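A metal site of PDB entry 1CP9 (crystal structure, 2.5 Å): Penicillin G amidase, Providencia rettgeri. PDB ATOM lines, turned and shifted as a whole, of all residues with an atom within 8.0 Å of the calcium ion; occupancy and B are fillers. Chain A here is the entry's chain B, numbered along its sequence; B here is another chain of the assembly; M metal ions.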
ATOM      1  N   GLY A  72      -5.340 -18.377   6.626  1.00  0.00           N
ATOM      2  CA  GLY A  72      -5.629 -17.350   5.637  1.00  0.00           C
ATOM      3  C   GLY A  72      -6.776 -16.530   6.237  1.00  0.00           C
ATOM      4  O   GLY A  72      -7.196 -16.774   7.389  1.00  0.00           O
ATOM      5  N   ASP A  73      -7.301 -15.567   5.494  1.00  0.00           N
ATOM      6  CA  ASP A  73      -8.387 -14.742   6.017  1.00  0.00           C
ATOM      7  C   ASP A  73      -9.681 -14.880   5.214  1.00  0.00           C
ATOM      8  O   ASP A  73      -9.890 -14.143   4.232  1.00  0.00           O
ATOM      9  CB  ASP A  73      -7.939 -13.266   6.092  1.00  0.00           C
ATOM     10  CG  ASP A  73      -9.015 -12.348   6.715  1.00  0.00           C
ATOM     11  OD1 ASP A  73     -10.159 -12.792   6.955  1.00  0.00           O
ATOM     12  OD2 ASP A  73      -8.697 -11.163   6.950  1.00  0.00           O
ATOM     13  N   GLY A  74     -10.557 -15.788   5.645  1.00  0.00           N
ATOM     14  CA  GLY A  74     -11.821 -15.988   4.975  1.00  0.00           C
ATOM     15  C   GLY A  74     -13.013 -15.651   5.872  1.00  0.00           C
ATOM     16  O   GLY A  74     -14.112 -16.132   5.628  1.00  0.00           O
ATOM     17  N   VAL A  75     -12.806 -14.793   6.868  1.00  0.00           N
ATOM     18  CA  VAL A  75     -13.842 -14.398   7.847  1.00  0.00           C
ATOM     19  C   VAL A  75     -13.707 -12.877   8.194  1.00  0.00           C
ATOM     20  O   VAL A  75     -12.724 -12.450   8.813  1.00  0.00           O
ATOM     21  CB  VAL A  75     -13.634 -15.217   9.155  1.00  0.00           C
ATOM     22  CG1 VAL A  75     -14.625 -14.787  10.251  1.00  0.00           C
ATOM     23  CG2 VAL A  75     -13.694 -16.678   8.847  1.00  0.00           C
ATOM     24  N   ASP A  76     -14.701 -12.075   7.803  1.00  0.00           N
ATOM     25  CA  ASP A  76     -14.695 -10.629   8.076  1.00  0.00           C
ATOM     26  C   ASP A  76     -15.865 -10.305   8.989  1.00  0.00           C
ATOM     27  O   ASP A  76     -16.830 -11.051   9.018  1.00  0.00           O
ATOM     28  CB  ASP A  76     -14.850  -9.806   6.794  1.00  0.00           C
ATOM     29  CG  ASP A  76     -13.694  -9.920   5.867  1.00  0.00           C
ATOM     30  OD1 ASP A  76     -12.586 -10.259   6.301  1.00  0.00           O
ATOM     31  OD2 ASP A  76     -13.880  -9.681   4.667  1.00  0.00           O
ATOM     32  N   ILE A  77     -15.761  -9.200   9.747  1.00  0.00           N
ATOM     33  CA  ILE A  77     -16.843  -8.719  10.635  1.00  0.00           C
ATOM     34  C   ILE A  77     -17.615  -7.587   9.880  1.00  0.00           C
ATOM     35  O   ILE A  77     -16.997  -6.749   9.214  1.00  0.00           O
ATOM     36  CB  ILE A  77     -16.304  -8.133  11.949  1.00  0.00           C
ATOM     37  CG1 ILE A  77     -15.487  -9.189  12.687  1.00  0.00           C
ATOM     38  CG2 ILE A  77     -17.427  -7.674  12.836  1.00  0.00           C
ATOM     39  CD1 ILE A  77     -16.245 -10.464  12.934  1.00  0.00           C
ATOM     40  N   ALA A 140     -19.106 -12.888   8.884  1.00  0.00           N
ATOM     41  CA  ALA A 140     -19.249 -13.443   7.548  1.00  0.00           C
ATOM     42  C   ALA A 140     -18.107 -14.403   7.270  1.00  0.00           C
ATOM     43  O   ALA A 140     -16.946 -14.037   7.411  1.00  0.00           O
ATOM     44  CB  ALA A 140     -19.269 -12.329   6.511  1.00  0.00           C
ATOM     45  N   PRO A 197     -12.812 -14.445   0.206  1.00  0.00           N
ATOM     46  CA  PRO A 197     -13.637 -13.403  -0.401  1.00  0.00           C
ATOM     47  C   PRO A 197     -12.961 -12.535  -1.439  1.00  0.00           C
ATOM     48  O   PRO A 197     -11.756 -12.332  -1.381  1.00  0.00           O
ATOM     49  CB  PRO A 197     -14.063 -12.547   0.792  1.00  0.00           C
ATOM     50  CG  PRO A 197     -13.045 -12.817   1.816  1.00  0.00           C
ATOM     51  CD  PRO A 197     -12.737 -14.269   1.658  1.00  0.00           C
ATOM     52  N   ARG A 199     -13.133  -9.201  -2.059  1.00  0.00           N
ATOM     53  CA  ARG A 199     -13.586  -8.002  -1.351  1.00  0.00           C
ATOM     54  C   ARG A 199     -13.627  -6.711  -2.156  1.00  0.00           C
ATOM     55  O   ARG A 199     -12.905  -6.548  -3.147  1.00  0.00           O
ATOM     56  CB  ARG A 199     -12.687  -7.770  -0.123  1.00  0.00           C
ATOM     57  CG  ARG A 199     -12.632  -8.944   0.871  1.00  0.00           C
ATOM     58  CD  ARG A 199     -11.660  -8.681   1.970  1.00  0.00           C
ATOM     59  NE  ARG A 199     -11.694  -9.700   3.027  1.00  0.00           N
ATOM     60  CZ  ARG A 199     -10.924 -10.787   3.090  1.00  0.00           C
ATOM     61  NH1 ARG A 199     -10.034 -11.063   2.146  1.00  0.00           N
ATOM     62  NH2 ARG A 199     -11.015 -11.616   4.118  1.00  0.00           N
ATOM     63  N   HIS A 203     -11.387  -2.512   1.170  1.00  0.00           N
ATOM     64  CA  HIS A 203     -11.996  -3.133   2.340  1.00  0.00           C
ATOM     65  C   HIS A 203     -10.778  -3.660   3.124  1.00  0.00           C
ATOM     66  O   HIS A 203      -9.990  -4.461   2.594  1.00  0.00           O
ATOM     67  CB  HIS A 203     -12.920  -4.283   1.865  1.00  0.00           C
ATOM     68  CG  HIS A 203     -13.408  -5.199   2.947  1.00  0.00           C
ATOM     69  ND1 HIS A 203     -14.221  -6.281   2.680  1.00  0.00           N
ATOM     70  CD2 HIS A 203     -13.199  -5.209   4.288  1.00  0.00           C
ATOM     71  CE1 HIS A 203     -14.485  -6.912   3.807  1.00  0.00           C
ATOM     72  NE2 HIS A 203     -13.878  -6.287   4.799  1.00  0.00           N
ATOM     73  N   ASP A 204     -10.550  -3.117   4.318  1.00  0.00           N
ATOM     74  CA  ASP A 204      -9.460  -3.595   5.148  1.00  0.00           C
ATOM     75  C   ASP A 204      -9.985  -4.860   5.820  1.00  0.00           C
ATOM     76  O   ASP A 204     -10.865  -4.807   6.697  1.00  0.00           O
ATOM     77  CB  ASP A 204      -9.058  -2.574   6.220  1.00  0.00           C
ATOM     78  CG  ASP A 204      -7.641  -2.833   6.771  1.00  0.00           C
ATOM     79  OD1 ASP A 204      -7.316  -3.982   7.066  1.00  0.00           O
ATOM     80  OD2 ASP A 204      -6.829  -1.889   6.850  1.00  0.00           O
ATOM     81  N   PRO A 205      -9.421  -6.022   5.462  1.00  0.00           N
ATOM     82  CA  PRO A 205      -9.908  -7.268   6.062  1.00  0.00           C
ATOM     83  C   PRO A 205      -9.561  -7.422   7.491  1.00  0.00           C
ATOM     84  O   PRO A 205      -9.980  -8.389   8.118  1.00  0.00           O
ATOM     85  CB  PRO A 205      -9.250  -8.343   5.199  1.00  0.00           C
ATOM     86  CG  PRO A 205      -7.956  -7.704   4.787  1.00  0.00           C
ATOM     87  CD  PRO A 205      -8.337  -6.293   4.485  1.00  0.00           C
ATOM     88  N   ARG A 206      -8.811  -6.456   8.028  1.00  0.00           N
ATOM     89  CA  ARG A 206      -8.371  -6.494   9.427  1.00  0.00           C
ATOM     90  C   ARG A 206      -9.293  -5.803  10.403  1.00  0.00           C
ATOM     91  O   ARG A 206      -9.141  -5.936  11.606  1.00  0.00           O
ATOM     92  CB  ARG A 206      -6.971  -5.900   9.583  1.00  0.00           C
ATOM     93  CG  ARG A 206      -5.867  -6.582   8.781  1.00  0.00           C
ATOM     94  CD  ARG A 206      -4.566  -5.817   8.988  1.00  0.00           C
ATOM     95  NE  ARG A 206      -4.659  -4.509   8.363  1.00  0.00           N
ATOM     96  CZ  ARG A 206      -3.796  -3.501   8.481  1.00  0.00           C
ATOM     97  NH1 ARG A 206      -2.701  -3.604   9.222  1.00  0.00           N
ATOM     98  NH2 ARG A 206      -4.074  -2.334   7.895  1.00  0.00           N
ATOM     99  N   LEU A 207     -10.269  -5.065   9.878  1.00  0.00           N
ATOM    100  CA  LEU A 207     -11.191  -4.308  10.723  1.00  0.00           C
ATOM    101  C   LEU A 207     -12.592  -4.451  10.210  1.00  0.00           C
ATOM    102  O   LEU A 207     -12.787  -4.881   9.086  1.00  0.00           O
ATOM    103  CB  LEU A 207     -10.758  -2.826  10.729  1.00  0.00           C
ATOM    104  CG  LEU A 207      -9.417  -2.472  11.404  1.00  0.00           C
ATOM    105  CD1 LEU A 207      -8.933  -1.225  10.790  1.00  0.00           C
ATOM    106  CD2 LEU A 207      -9.572  -2.337  12.907  1.00  0.00           C
ATOM    107  N   PRO A 208     -13.607  -4.205  11.054  1.00  0.00           N
ATOM    108  CA  PRO A 208     -14.988  -4.335  10.583  1.00  0.00           C
ATOM    109  C   PRO A 208     -15.255  -3.364   9.425  1.00  0.00           C
ATOM    110  O   PRO A 208     -14.517  -2.383   9.241  1.00  0.00           O
ATOM    111  CB  PRO A 208     -15.812  -3.924  11.795  1.00  0.00           C
ATOM    112  CG  PRO A 208     -14.955  -4.287  12.960  1.00  0.00           C
ATOM    113  CD  PRO A 208     -13.558  -3.894  12.503  1.00  0.00           C
ATOM    114  N   TRP A 217     -18.979  -8.586  -0.021  1.00  0.00           N
ATOM    115  CA  TRP A 217     -18.039  -9.249  -0.903  1.00  0.00           C
ATOM    116  C   TRP A 217     -18.629  -9.330  -2.311  1.00  0.00           C
ATOM    117  O   TRP A 217     -19.830  -9.516  -2.492  1.00  0.00           O
ATOM    118  CB  TRP A 217     -17.775 -10.660  -0.424  1.00  0.00           C
ATOM    119  CG  TRP A 217     -17.176 -10.731   0.938  1.00  0.00           C
ATOM    120  CD1 TRP A 217     -16.482  -9.746   1.605  1.00  0.00           C
ATOM    121  CD2 TRP A 217     -17.179 -11.872   1.796  1.00  0.00           C
ATOM    122  NE1 TRP A 217     -16.048 -10.204   2.813  1.00  0.00           N
ATOM    123  CE2 TRP A 217     -16.459 -11.516   2.956  1.00  0.00           C
ATOM    124  CE3 TRP A 217     -17.717 -13.160   1.699  1.00  0.00           C
ATOM    125  CZ2 TRP A 217     -16.268 -12.406   4.022  1.00  0.00           C
ATOM    126  CZ3 TRP A 217     -17.535 -14.032   2.753  1.00  0.00           C
ATOM    127  CH2 TRP A 217     -16.807 -13.658   3.899  1.00  0.00           C
ATOM    128  N   ALA A 250      -2.347 -13.265   5.884  1.00  0.00           N
ATOM    129  CA  ALA A 250      -2.788 -14.117   6.954  1.00  0.00           C
ATOM    130  C   ALA A 250      -4.102 -13.560   7.506  1.00  0.00           C
ATOM    131  O   ALA A 250      -4.576 -12.487   7.068  1.00  0.00           O
ATOM    132  CB  ALA A 250      -1.705 -14.127   8.070  1.00  0.00           C
ATOM    133  N   SER A 251      -4.685 -14.302   8.428  1.00  0.00           N
ATOM    134  CA  SER A 251      -5.878 -13.923   9.155  1.00  0.00           C
ATOM    135  C   SER A 251      -5.617 -12.588   9.872  1.00  0.00           C
ATOM    136  O   SER A 251      -4.506 -12.298  10.299  1.00  0.00           O
ATOM    137  CB  SER A 251      -6.156 -14.986  10.244  1.00  0.00           C
ATOM    138  OG  SER A 251      -7.048 -14.492  11.260  1.00  0.00           O
ATOM    139  N   ASP A 252      -6.694 -11.850  10.123  1.00  0.00           N
ATOM    140  CA  ASP A 252      -6.662 -10.571  10.803  1.00  0.00           C
ATOM    141  C   ASP A 252      -6.235 -10.657  12.273  1.00  0.00           C
ATOM    142  O   ASP A 252      -5.989  -9.613  12.901  1.00  0.00           O
ATOM    143  CB  ASP A 252      -8.041  -9.937  10.737  1.00  0.00           C
ATOM    144  CG  ASP A 252      -9.161 -10.928  11.073  1.00  0.00           C
ATOM    145  OD1 ASP A 252      -9.666 -11.592  10.136  1.00  0.00           O
ATOM    146  OD2 ASP A 252      -9.553 -11.023  12.255  1.00  0.00           O
ATOM    147  N   LEU A 253      -6.259 -11.868  12.838  1.00  0.00           N
ATOM    148  CA  LEU A 253      -5.871 -12.122  14.242  1.00  0.00           C
ATOM    149  C   LEU A 253      -4.647 -11.275  14.640  1.00  0.00           C
ATOM    150  O   LEU A 253      -3.611 -11.314  13.956  1.00  0.00           O
ATOM    151  CB  LEU A 253      -5.524 -13.599  14.421  1.00  0.00           C
ATOM    152  CG  LEU A 253      -6.561 -14.602  14.898  1.00  0.00           C
ATOM    153  CD1 LEU A 253      -5.849 -15.877  15.296  1.00  0.00           C
ATOM    154  CD2 LEU A 253      -7.288 -14.040  16.104  1.00  0.00           C
ATOM    155  N   MET B 147     -11.363 -18.129  13.382  1.00  0.00           N
ATOM    156  CA  MET B 147     -10.636 -17.149  14.186  1.00  0.00           C
ATOM    157  C   MET B 147     -10.803 -15.782  13.560  1.00  0.00           C
ATOM    158  O   MET B 147     -10.881 -15.661  12.340  1.00  0.00           O
ATOM    159  CB  MET B 147      -9.151 -17.504  14.322  1.00  0.00           C
ATOM    160  CG  MET B 147      -8.421 -17.739  13.009  1.00  0.00           C
ATOM    161  SD  MET B 147      -8.502 -19.424  12.394  1.00  0.00           S
ATOM    162  CE  MET B 147      -7.655 -19.116  10.775  1.00  0.00           C
ATOM    163  N   ASN B 148     -10.830 -14.756  14.410  1.00  0.00           N
ATOM    164  CA  ASN B 148     -11.011 -13.383  13.975  1.00  0.00           C
ATOM    165  C   ASN B 148     -10.845 -12.455  15.197  1.00  0.00           C
ATOM    166  O   ASN B 148     -11.294 -12.777  16.304  1.00  0.00           O
ATOM    167  CB  ASN B 148     -12.424 -13.270  13.410  1.00  0.00           C
ATOM    168  CG  ASN B 148     -12.745 -11.895  12.904  1.00  0.00           C
ATOM    169  OD1 ASN B 148     -13.062 -10.994  13.686  1.00  0.00           O
ATOM    170  ND2 ASN B 148     -12.654 -11.696  11.576  1.00  0.00           N
ATOM    171  N   SER B 149     -10.171 -11.313  15.026  1.00  0.00           N
ATOM    172  CA  SER B 149     -10.015 -10.370  16.142  1.00  0.00           C
ATOM    173  C   SER B 149     -10.260  -8.948  15.646  1.00  0.00           C
ATOM    174  O   SER B 149      -9.806  -7.990  16.258  1.00  0.00           O
ATOM    175  CB  SER B 149      -8.638 -10.480  16.795  1.00  0.00           C
ATOM    176  OG  SER B 149      -7.622  -9.929  15.953  1.00  0.00           O
ATOM    177  N   GLU B 150     -11.042  -8.807  14.589  1.00  0.00           N
ATOM    178  CA  GLU B 150     -11.348  -7.503  14.022  1.00  0.00           C
ATOM    179  C   GLU B 150     -11.958  -6.455  14.966  1.00  0.00           C
ATOM    180  O   GLU B 150     -11.667  -5.280  14.836  1.00  0.00           O
ATOM    181  CB  GLU B 150     -12.204  -7.668  12.792  1.00  0.00           C
ATOM    182  CG  GLU B 150     -11.498  -8.355  11.680  1.00  0.00           C
ATOM    183  CD  GLU B 150     -12.393  -8.577  10.475  1.00  0.00           C
ATOM    184  OE1 GLU B 150     -13.381  -7.828  10.331  1.00  0.00           O
ATOM    185  OE2 GLU B 150     -12.120  -9.498   9.678  1.00  0.00           O
ATOM    186  N   ASN B 153      -9.119  -5.423  17.142  1.00  0.00           N
ATOM    187  CA  ASN B 153      -8.223  -4.677  16.285  1.00  0.00           C
ATOM    188  C   ASN B 153      -8.725  -3.229  16.179  1.00  0.00           C
ATOM    189  O   ASN B 153      -7.918  -2.297  16.143  1.00  0.00           O
ATOM    190  CB  ASN B 153      -8.178  -5.285  14.877  1.00  0.00           C
ATOM    191  CG  ASN B 153      -7.389  -6.568  14.808  1.00  0.00           C
ATOM    192  OD1 ASN B 153      -6.874  -7.085  15.820  1.00  0.00           O
ATOM    193  ND2 ASN B 153      -7.315  -7.114  13.617  1.00  0.00           N
ATOM    194  N   LEU B 179      -0.636  -6.494   6.995  1.00  0.00           N
ATOM    195  CA  LEU B 179      -1.454  -7.346   6.156  1.00  0.00           C
ATOM    196  C   LEU B 179      -0.495  -8.455   5.721  1.00  0.00           C
ATOM    197  O   LEU B 179      -0.846  -9.645   5.732  1.00  0.00           O
ATOM    198  CB  LEU B 179      -1.951  -6.550   4.957  1.00  0.00           C
ATOM    199  CG  LEU B 179      -3.367  -6.769   4.383  1.00  0.00           C
ATOM    200  CD1 LEU B 179      -4.333  -7.550   5.323  1.00  0.00           C
ATOM    201  CD2 LEU B 179      -3.893  -5.370   4.117  1.00  0.00           C
HETATM  202 CA    CA M   1     -10.818 -10.809   8.180  1.00  0.00          CA
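The backbone carbonyl oxygen (O) of Asp 252 lies within hydrogen-bond range of the side-chain amide nitrogen (ND2) of Asn 153 of chain B (2.9 Å). OD2 of Asp 76 lies close to NE2 of His 203, at 3.4 Å. OD2 of Asp 76 is in salt-bridge range of NE of Arg 199, 2.7 Å away. O of Asp 73 is in hydrogen-bond range of NH2 of Arg 199 (2.8 Å). The side-chain carboxylate of Asp 252 lies within hydrogen-bond range of the backbone NH of Ser 149 of chain B, 2.9 Å away. The backbone NH (N) of Ala 140 is in hydrogen-bond range of the backbone carbonyl oxygen (O) of Asp 76 (2.9 Å). O of Val 75 lies close to ND2 of Asn 148 of chain B, at 2.9 Å. The side-chain amide oxygen (OD1) of Asn 148 of chain B sits at hydrogen-bond distance from the backbone NH (N) of Glu 150 of chain B, 3.1 Å away.
Asn 148 of chain B touches the calcium ion. The nearest printed residue that does not touch the calcium ion is Arg 199 (4.1 Å).
OE2 of Glu 150 of chain B is bound to the calcium ion (2.4 Å). OD1 of Asp 252 binds the calcium ion, at 2.4 Å. OD1 of Asp 73 is bound to the calcium ion (2.4 Å). The calcium ion is bound by OD2 of Asp 73 (2.5 Å). The calcium ion is bound by the backbone carbonyl oxygen (O) of Pro 205 (2.6 Å). The backbone carbonyl oxygen (O) of Val 75 is bound to the calcium ion (2.6 Å). OD1 of Asp 76 binds the calcium ion, at 2.6 Å. The calcium ion has seven donor atoms within binding distance.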
